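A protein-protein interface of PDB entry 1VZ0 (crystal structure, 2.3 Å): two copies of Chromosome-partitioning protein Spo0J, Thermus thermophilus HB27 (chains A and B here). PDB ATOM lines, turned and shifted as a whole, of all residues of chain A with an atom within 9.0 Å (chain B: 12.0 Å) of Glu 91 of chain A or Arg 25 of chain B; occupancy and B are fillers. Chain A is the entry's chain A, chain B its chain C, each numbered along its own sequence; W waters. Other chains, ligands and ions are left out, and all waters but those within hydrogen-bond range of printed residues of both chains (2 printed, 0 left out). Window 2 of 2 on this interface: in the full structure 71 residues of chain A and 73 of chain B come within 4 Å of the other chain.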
ATOM      1  N   ILE A  54       5.775 -26.014  -6.118  1.00  0.00           N
ATOM      2  CA  ILE A  54       4.977 -24.967  -6.741  1.00  0.00           C
ATOM      3  C   ILE A  54       4.703 -25.302  -8.214  1.00  0.00           C
ATOM      4  O   ILE A  54       3.680 -24.911  -8.757  1.00  0.00           O
ATOM      5  CB  ILE A  54       5.662 -23.586  -6.626  1.00  0.00           C
ATOM      6  CG1 ILE A  54       5.585 -23.096  -5.175  1.00  0.00           C
ATOM      7  CG2 ILE A  54       4.983 -22.580  -7.564  1.00  0.00           C
ATOM      8  CD1 ILE A  54       6.285 -21.763  -4.921  1.00  0.00           C
ATOM      9  N   GLY A  58       1.257 -24.854  -7.556  1.00  0.00           N
ATOM     10  CA  GLY A  58       1.066 -23.420  -7.643  1.00  0.00           C
ATOM     11  C   GLY A  58       1.311 -22.852  -6.256  1.00  0.00           C
ATOM     12  O   GLY A  58       1.766 -23.572  -5.364  1.00  0.00           O
ATOM     13  N   LEU A  59       1.024 -21.573  -6.061  1.00  0.00           N
ATOM     14  CA  LEU A  59       1.227 -20.966  -4.758  1.00  0.00           C
ATOM     15  C   LEU A  59       0.075 -21.300  -3.835  1.00  0.00           C
ATOM     16  O   LEU A  59      -1.085 -21.264  -4.238  1.00  0.00           O
ATOM     17  CB  LEU A  59       1.342 -19.448  -4.874  1.00  0.00           C
ATOM     18  CG  LEU A  59       2.595 -18.894  -5.552  1.00  0.00           C
ATOM     19  CD1 LEU A  59       2.595 -17.376  -5.488  1.00  0.00           C
ATOM     20  CD2 LEU A  59       3.816 -19.441  -4.842  1.00  0.00           C
ATOM     21  N   PRO A  62      -1.316 -16.226  -1.975  1.00  0.00           N
ATOM     22  CA  PRO A  62      -0.928 -15.141  -2.884  1.00  0.00           C
ATOM     23  C   PRO A  62       0.252 -14.365  -2.325  1.00  0.00           C
ATOM     24  O   PRO A  62       0.521 -14.396  -1.122  1.00  0.00           O
ATOM     25  CB  PRO A  62      -2.180 -14.261  -2.942  1.00  0.00           C
ATOM     26  CG  PRO A  62      -3.298 -15.228  -2.654  1.00  0.00           C
ATOM     27  CD  PRO A  62      -2.722 -16.090  -1.554  1.00  0.00           C
ATOM     28  N   LEU A  63       0.961 -13.677  -3.202  1.00  0.00           N
ATOM     29  CA  LEU A  63       2.071 -12.848  -2.776  1.00  0.00           C
ATOM     30  C   LEU A  63       1.442 -11.511  -2.407  1.00  0.00           C
ATOM     31  O   LEU A  63       0.401 -11.147  -2.952  1.00  0.00           O
ATOM     32  CB  LEU A  63       3.054 -12.641  -3.926  1.00  0.00           C
ATOM     33  CG  LEU A  63       3.689 -13.874  -4.573  1.00  0.00           C
ATOM     34  CD1 LEU A  63       4.605 -13.423  -5.684  1.00  0.00           C
ATOM     35  CD2 LEU A  63       4.457 -14.679  -3.525  1.00  0.00           C
ATOM     36  N   VAL A  65       1.911  -7.591  -2.589  1.00  0.00           N
ATOM     37  CA  VAL A  65       2.729  -6.615  -3.287  1.00  0.00           C
ATOM     38  C   VAL A  65       2.112  -5.223  -3.297  1.00  0.00           C
ATOM     39  O   VAL A  65       0.924  -5.034  -2.997  1.00  0.00           O
ATOM     40  CB  VAL A  65       2.982  -7.034  -4.760  1.00  0.00           C
ATOM     41  CG1 VAL A  65       3.530  -8.453  -4.815  1.00  0.00           C
ATOM     42  CG2 VAL A  65       1.696  -6.933  -5.569  1.00  0.00           C
ATOM     43  N   TYR A  72       5.350  -3.837  -9.880  1.00  0.00           N
ATOM     44  CA  TYR A  72       5.038  -4.020  -8.469  1.00  0.00           C
ATOM     45  C   TYR A  72       6.254  -4.468  -7.670  1.00  0.00           C
ATOM     46  O   TYR A  72       7.227  -5.001  -8.210  1.00  0.00           O
ATOM     47  CB  TYR A  72       3.929  -5.051  -8.284  1.00  0.00           C
ATOM     48  CG  TYR A  72       2.722  -4.832  -9.159  1.00  0.00           C
ATOM     49  CD1 TYR A  72       2.688  -5.317 -10.464  1.00  0.00           C
ATOM     50  CD2 TYR A  72       1.629  -4.116  -8.699  1.00  0.00           C
ATOM     51  CE1 TYR A  72       1.597  -5.087 -11.290  1.00  0.00           C
ATOM     52  CE2 TYR A  72       0.530  -3.881  -9.515  1.00  0.00           C
ATOM     53  CZ  TYR A  72       0.524  -4.366 -10.812  1.00  0.00           C
ATOM     54  OH  TYR A  72      -0.546  -4.108 -11.640  1.00  0.00           O
ATOM     55  N   ALA A  84       8.901 -19.426  -6.843  1.00  0.00           N
ATOM     56  CA  ALA A  84       8.062 -19.313  -8.037  1.00  0.00           C
ATOM     57  C   ALA A  84       8.941 -19.033  -9.256  1.00  0.00           C
ATOM     58  O   ALA A  84       8.744 -19.616 -10.327  1.00  0.00           O
ATOM     59  CB  ALA A  84       7.021 -18.202  -7.861  1.00  0.00           C
ATOM     60  N   LEU A  85       9.910 -18.141  -9.086  1.00  0.00           N
ATOM     61  CA  LEU A  85      10.826 -17.813 -10.172  1.00  0.00           C
ATOM     62  C   LEU A  85      11.574 -19.084 -10.582  1.00  0.00           C
ATOM     63  O   LEU A  85      11.658 -19.404 -11.765  1.00  0.00           O
ATOM     64  CB  LEU A  85      11.814 -16.725  -9.724  1.00  0.00           C
ATOM     65  CG  LEU A  85      11.193 -15.334  -9.552  1.00  0.00           C
ATOM     66  CD1 LEU A  85      12.187 -14.365  -8.907  1.00  0.00           C
ATOM     67  CD2 LEU A  85      10.750 -14.820 -10.920  1.00  0.00           C
ATOM     68  N   ALA A  87      10.639 -22.039 -10.233  1.00  0.00           N
ATOM     69  CA  ALA A  87       9.661 -22.949 -10.817  1.00  0.00           C
ATOM     70  C   ALA A  87       9.325 -22.619 -12.266  1.00  0.00           C
ATOM     71  O   ALA A  87       8.689 -23.422 -12.946  1.00  0.00           O
ATOM     72  CB  ALA A  87       8.379 -22.941  -9.979  1.00  0.00           C
ATOM     73  N   GLY A  88       9.733 -21.438 -12.725  1.00  0.00           N
ATOM     74  CA  GLY A  88       9.454 -21.041 -14.094  1.00  0.00           C
ATOM     75  C   GLY A  88       8.033 -20.556 -14.352  1.00  0.00           C
ATOM     76  O   GLY A  88       7.597 -20.503 -15.507  1.00  0.00           O
ATOM     77  N   LEU A  89       7.295 -20.205 -13.300  1.00  0.00           N
ATOM     78  CA  LEU A  89       5.940 -19.717 -13.496  1.00  0.00           C
ATOM     79  C   LEU A  89       5.982 -18.337 -14.160  1.00  0.00           C
ATOM     80  O   LEU A  89       6.891 -17.544 -13.916  1.00  0.00           O
ATOM     81  CB  LEU A  89       5.196 -19.620 -12.156  1.00  0.00           C
ATOM     82  CG  LEU A  89       5.019 -20.916 -11.347  1.00  0.00           C
ATOM     83  CD1 LEU A  89       4.134 -20.654 -10.135  1.00  0.00           C
ATOM     84  CD2 LEU A  89       4.409 -21.990 -12.231  1.00  0.00           C
ATOM     85  N   GLN A  90       5.004 -18.064 -15.016  1.00  0.00           N
ATOM     86  CA  GLN A  90       4.923 -16.774 -15.682  1.00  0.00           C
ATOM     87  C   GLN A  90       4.074 -15.837 -14.831  1.00  0.00           C
ATOM     88  O   GLN A  90       4.340 -14.644 -14.755  1.00  0.00           O
ATOM     89  CB  GLN A  90       4.286 -16.907 -17.073  1.00  0.00           C
ATOM     90  CG  GLN A  90       5.169 -17.552 -18.131  1.00  0.00           C
ATOM     91  CD  GLN A  90       4.631 -17.345 -19.550  1.00  0.00           C
ATOM     92  OE1 GLN A  90       5.101 -17.970 -20.506  1.00  0.00           O
ATOM     93  NE2 GLN A  90       3.645 -16.458 -19.690  1.00  0.00           N
ATOM     94  N   GLU A  91       3.048 -16.393 -14.196  1.00  0.00           N
ATOM     95  CA  GLU A  91       2.139 -15.618 -13.360  1.00  0.00           C
ATOM     96  C   GLU A  91       1.948 -16.270 -12.002  1.00  0.00           C
ATOM     97  O   GLU A  91       2.156 -17.474 -11.841  1.00  0.00           O
ATOM     98  CB  GLU A  91       0.777 -15.487 -14.043  1.00  0.00           C
ATOM     99  CG  GLU A  91       0.787 -14.656 -15.312  1.00  0.00           C
ATOM    100  CD  GLU A  91      -0.500 -14.797 -16.106  1.00  0.00           C
ATOM    101  OE1 GLU A  91      -0.677 -14.058 -17.100  1.00  0.00           O
ATOM    102  OE2 GLU A  91      -1.329 -15.655 -15.736  1.00  0.00           O
ATOM    103  N   VAL A  92       1.536 -15.465 -11.032  1.00  0.00           N
ATOM    104  CA  VAL A  92       1.295 -15.946  -9.685  1.00  0.00           C
ATOM    105  C   VAL A  92       0.144 -15.163  -9.072  1.00  0.00           C
ATOM    106  O   VAL A  92      -0.136 -14.029  -9.470  1.00  0.00           O
ATOM    107  CB  VAL A  92       2.539 -15.763  -8.788  1.00  0.00           C
ATOM    108  CG1 VAL A  92       3.662 -16.694  -9.236  1.00  0.00           C
ATOM    109  CG2 VAL A  92       3.004 -14.316  -8.840  1.00  0.00           C
ATOM    110  N   PRO A  93      -0.574 -15.776  -8.125  1.00  0.00           N
ATOM    111  CA  PRO A  93      -1.682 -15.065  -7.484  1.00  0.00           C
ATOM    112  C   PRO A  93      -1.074 -14.014  -6.560  1.00  0.00           C
ATOM    113  O   PRO A  93      -0.002 -14.225  -5.991  1.00  0.00           O
ATOM    114  CB  PRO A  93      -2.408 -16.172  -6.715  1.00  0.00           C
ATOM    115  CG  PRO A  93      -1.306 -17.172  -6.428  1.00  0.00           C
ATOM    116  CD  PRO A  93      -0.560 -17.197  -7.740  1.00  0.00           C
ATOM    117  N   ALA A  94      -1.737 -12.877  -6.412  1.00  0.00           N
ATOM    118  CA  ALA A  94      -1.198 -11.839  -5.547  1.00  0.00           C
ATOM    119  C   ALA A  94      -2.272 -10.899  -5.043  1.00  0.00           C
ATOM    120  O   ALA A  94      -3.376 -10.849  -5.584  1.00  0.00           O
ATOM    121  CB  ALA A  94      -0.121 -11.044  -6.291  1.00  0.00           C
ATOM    122  N   VAL A  95      -1.943 -10.172  -3.983  1.00  0.00           N
ATOM    123  CA  VAL A  95      -2.851  -9.190  -3.422  1.00  0.00           C
ATOM    124  C   VAL A  95      -2.099  -7.876  -3.488  1.00  0.00           C
ATOM    125  O   VAL A  95      -0.984  -7.759  -2.983  1.00  0.00           O
ATOM    126  CB  VAL A  95      -3.218  -9.504  -1.946  1.00  0.00           C
ATOM    127  CG1 VAL A  95      -4.025  -8.344  -1.349  1.00  0.00           C
ATOM    128  CG2 VAL A  95      -4.038 -10.785  -1.879  1.00  0.00           C
ATOM    129  N   VAL A  96      -2.708  -6.892  -4.136  1.00  0.00           N
ATOM    130  CA  VAL A  96      -2.098  -5.577  -4.274  1.00  0.00           C
ATOM    131  C   VAL A  96      -2.644  -4.599  -3.245  1.00  0.00           C
ATOM    132  O   VAL A  96      -3.852  -4.465  -3.094  1.00  0.00           O
ATOM    133  CB  VAL A  96      -2.379  -4.979  -5.658  1.00  0.00           C
ATOM    134  CG1 VAL A  96      -1.622  -3.653  -5.825  1.00  0.00           C
ATOM    135  CG2 VAL A  96      -2.004  -5.973  -6.730  1.00  0.00           C
ATOM    136  N   VAL B  23      -7.730 -10.405  -4.843  1.00  0.00           N
ATOM    137  CA  VAL B  23      -6.684 -11.336  -5.385  1.00  0.00           C
ATOM    138  C   VAL B  23      -6.661 -11.328  -6.907  1.00  0.00           C
ATOM    139  O   VAL B  23      -7.678 -11.562  -7.551  1.00  0.00           O
ATOM    140  CB  VAL B  23      -6.924 -12.797  -4.938  1.00  0.00           C
ATOM    141  CG1 VAL B  23      -5.876 -13.704  -5.545  1.00  0.00           C
ATOM    142  CG2 VAL B  23      -6.878 -12.895  -3.432  1.00  0.00           C
ATOM    143  N   VAL B  24      -5.490 -11.078  -7.479  1.00  0.00           N
ATOM    144  CA  VAL B  24      -5.353 -11.043  -8.930  1.00  0.00           C
ATOM    145  C   VAL B  24      -4.157 -11.854  -9.398  1.00  0.00           C
ATOM    146  O   VAL B  24      -3.319 -12.264  -8.602  1.00  0.00           O
ATOM    147  CB  VAL B  24      -5.195  -9.592  -9.443  1.00  0.00           C
ATOM    148  CG1 VAL B  24      -6.433  -8.788  -9.092  1.00  0.00           C
ATOM    149  CG2 VAL B  24      -3.955  -8.947  -8.819  1.00  0.00           C
ATOM    150  N   ARG B  25      -4.085 -12.074 -10.701  1.00  0.00           N
ATOM    151  CA  ARG B  25      -3.008 -12.840 -11.292  1.00  0.00           C
ATOM    152  C   ARG B  25      -2.024 -11.870 -11.946  1.00  0.00           C
ATOM    153  O   ARG B  25      -2.368 -11.192 -12.917  1.00  0.00           O
ATOM    154  CB  ARG B  25      -3.608 -13.799 -12.314  1.00  0.00           C
ATOM    155  CG  ARG B  25      -2.681 -14.846 -12.881  1.00  0.00           C
ATOM    156  CD  ARG B  25      -3.491 -15.862 -13.703  1.00  0.00           C
ATOM    157  NE  ARG B  25      -3.557 -15.546 -15.132  1.00  0.00           N
ATOM    158  CZ  ARG B  25      -4.004 -14.403 -15.655  1.00  0.00           C
ATOM    159  NH1 ARG B  25      -4.010 -14.241 -16.974  1.00  0.00           N
ATOM    160  NH2 ARG B  25      -4.448 -13.423 -14.879  1.00  0.00           N
ATOM    161  N   LEU B  26      -0.808 -11.798 -11.406  1.00  0.00           N
ATOM    162  CA  LEU B  26       0.212 -10.894 -11.936  1.00  0.00           C
ATOM    163  C   LEU B  26       1.402 -11.631 -12.536  1.00  0.00           C
ATOM    164  O   LEU B  26       1.764 -12.716 -12.085  1.00  0.00           O
ATOM    165  CB  LEU B  26       0.733  -9.963 -10.830  1.00  0.00           C
ATOM    166  CG  LEU B  26      -0.218  -8.974 -10.149  1.00  0.00           C
ATOM    167  CD1 LEU B  26       0.510  -8.239  -9.020  1.00  0.00           C
ATOM    168  CD2 LEU B  26      -0.737  -7.983 -11.176  1.00  0.00           C
ATOM    169  N   PRO B  27       2.018 -11.058 -13.580  1.00  0.00           N
ATOM    170  CA  PRO B  27       3.179 -11.712 -14.191  1.00  0.00           C
ATOM    171  C   PRO B  27       4.372 -11.554 -13.263  1.00  0.00           C
ATOM    172  O   PRO B  27       4.620 -10.469 -12.734  1.00  0.00           O
ATOM    173  CB  PRO B  27       3.350 -10.969 -15.519  1.00  0.00           C
ATOM    174  CG  PRO B  27       2.721  -9.633 -15.264  1.00  0.00           C
ATOM    175  CD  PRO B  27       1.512  -9.969 -14.433  1.00  0.00           C
ATOM    176  N   LEU B  28       5.105 -12.643 -13.061  1.00  0.00           N
ATOM    177  CA  LEU B  28       6.253 -12.638 -12.174  1.00  0.00           C
ATOM    178  C   LEU B  28       7.266 -11.583 -12.598  1.00  0.00           C
ATOM    179  O   LEU B  28       7.864 -10.908 -11.755  1.00  0.00           O
ATOM    180  CB  LEU B  28       6.877 -14.041 -12.153  1.00  0.00           C
ATOM    181  CG  LEU B  28       7.423 -14.626 -10.849  1.00  0.00           C
ATOM    182  CD1 LEU B  28       6.591 -14.174  -9.666  1.00  0.00           C
ATOM    183  CD2 LEU B  28       7.419 -16.155 -10.939  1.00  0.00           C
ATOM    184  N   ALA B  29       7.429 -11.421 -13.907  1.00  0.00           N
ATOM    185  CA  ALA B  29       8.373 -10.451 -14.458  1.00  0.00           C
ATOM    186  C   ALA B  29       8.026  -9.012 -14.067  1.00  0.00           C
ATOM    187  O   ALA B  29       8.852  -8.109 -14.188  1.00  0.00           O
ATOM    188  CB  ALA B  29       8.427 -10.578 -15.972  1.00  0.00           C
ATOM    189  N   SER B  30       6.809  -8.788 -13.593  1.00  0.00           N
ATOM    190  CA  SER B  30       6.453  -7.441 -13.206  1.00  0.00           C
ATOM    191  C   SER B  30       6.452  -7.235 -11.681  1.00  0.00           C
ATOM    192  O   SER B  30       5.917  -6.250 -11.177  1.00  0.00           O
ATOM    193  CB  SER B  30       5.115  -7.040 -13.858  1.00  0.00           C
ATOM    194  OG  SER B  30       4.025  -7.713 -13.284  1.00  0.00           O
ATOM    195  N   ILE B  31       7.088  -8.160 -10.958  1.00  0.00           N
ATOM    196  CA  ILE B  31       7.197  -8.071  -9.502  1.00  0.00           C
ATOM    197  C   ILE B  31       8.681  -8.123  -9.120  1.00  0.00           C
ATOM    198  O   ILE B  31       9.350  -9.140  -9.328  1.00  0.00           O
ATOM    199  CB  ILE B  31       6.450  -9.240  -8.782  1.00  0.00           C
ATOM    200  CG1 ILE B  31       4.944  -9.145  -9.033  1.00  0.00           C
ATOM    201  CG2 ILE B  31       6.709  -9.177  -7.287  1.00  0.00           C
ATOM    202  CD1 ILE B  31       4.137 -10.356  -8.507  1.00  0.00           C
HETATM  203  O   HOH W   1       8.471  -4.650 -11.200  1.00  0.00           O
HETATM  204  O   HOH W   2       6.293 -13.024 -16.182  1.00  0.00           O
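O of Ser 30 of chain B sits at hydrogen-bond distance from N of Tyr 72 of chain A, at 2.8 Å. The backbone carbonyl oxygen (O) of Gln 90 of chain A sits at hydrogen-bond distance from the backbone NH (N) of Leu 28 of chain B (2.7 Å). The side-chain carboxylate of Glu 91 of chain A lies within salt-bridge range of the guanidinium group of Arg 25 of chain B (3.3 Å). The backbone NH (N) of Val 92 of chain A is in hydrogen-bond range of the backbone carbonyl oxygen (O) of Leu 26 of chain B. The backbone carbonyl oxygen (O) of Val 24 of chain B lies within hydrogen-bond range of the backbone NH (N) of Ala 94 of chain A (2.8 Å).
The backbone NH (N) of Leu 63 of chain A sits at hydrogen-bond distance from the backbone carbonyl oxygen (O) of Pro 93 of chain A (3.0 Å). The backbone carbonyl oxygen (O) of Leu 63 of chain A sits at hydrogen-bond distance from the backbone NH (N) of Val 95 of chain A (2.7 Å). The backbone NH (N) of Val 65 of chain A is in hydrogen-bond range of the backbone carbonyl oxygen (O) of Val 95 of chain A, at 2.9 Å. O of Ala 84 of chain A is in hydrogen-bond range of N of Leu 89 of chain A, 3.4 Å away. The side-chain hydroxyl (OG) of Ser 30 of chain B sits at hydrogen-bond distance from the backbone carbonyl oxygen (O) of Pro 27 of chain B, 2.9 Å away.
CD2 of Leu 85 of chain A touches CG of Leu 28 of chain B, at 3.3 Å. O of Leu 89 of chain A touches CD2 of Leu 28 of chain B, at 3.3 Å. Pro 27 of chain B touches Gln 90 of chain A (CA to O, 3.2 Å). CA of Glu 91 of chain A touches O of Leu 26 of chain B, at 3.2 Å. CG of Glu 91 of chain A touches CA of Pro 27 of chain B, at 3.96 Å. Val 92 of chain A touches Leu 28 of chain B. Pro 93 of chain A touches Val 24 of chain B. Ala 94 of chain A touches Val 23 of chain B (O to CA, 3.3 Å). Ala 94 of chain A touches Leu 26 of chain B. Val 23 of chain B touches Val 95 of chain A.
Ile 54 of chain A touches none of the printed residues of chain B. Pro 62 of chain A touches none of the printed residues of chain B. Printed residues of chain B within 4 Å of Val 65 of chain A: Leu 26. Of the printed residues of chain B, Leu 85 of chain A touches Leu 28. Of chain B, only Arg 25, Leu 26 and Pro 27 come within 4 Å of Glu 91 of chain A. Val 92 of chain A touches just these residues of chain B: Val 24, Arg 25, Leu 26 and Leu 28. Printed residues of chain B within 4 Å of Ala 94 of chain A: Val 23, Val 24 and Leu 26. Val 24 of chain B touches just these residues of chain A: Val 92, Pro 93 and Ala 94. Of the printed residues of chain A, Arg 25 of chain B touches Glu 91 (2.3 Å) and Val 92 (3.6 Å). Printed residues of chain A within 4 Å of Leu 28 of chain B: Ala 84, Leu 85, Leu 89, Gln 90 and Val 92. Printed residues of chain A within 4 Å of Ile 31 of chain B: Tyr 72. The nearest residue of chain A that does not touch Arg 25 of chain B is Pro 93 of chain A (4.6 Å). The nearest printed residue of chain B that does not touch Tyr 72 of chain A is Pro 27 of chain B (5.8 Å).
Of the 9 printed residues of chain B, 8 touch a printed residue of chain A. Of the 19 printed residues of chain A, 11 touch a printed residue of chain B. Hydrophobic or aromatic side chains of chain A within 4 Å of the printed part of chain B: Val 65, Tyr 72, Ala 84, Leu 85, Val 92, Ala 94 and Val 95. Among the printed residues, Asp or Glu carboxylates within 4 Å of a Lys or Arg side-chain nitrogen of the other chain: Glu 91 of chain A with Arg 25 of chain B.
No position is printed for both chains. Of the 21 pairs that touch across the chains among the printed residues, none has its exchanged pair printed and touching as well.
Water W2 lies within hydrogen-bond range of the backbone carbonyl oxygen of Gln 90 of chain A, the backbone NH of Ala 29 of chain B and the backbone NH of Leu 28 of chain B. Water W1 lies within hydrogen-bond range of the backbone carbonyl oxygen (O) of Ser 30 of chain B and the backbone carbonyl oxygen (O) of Tyr 72 of chain A.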
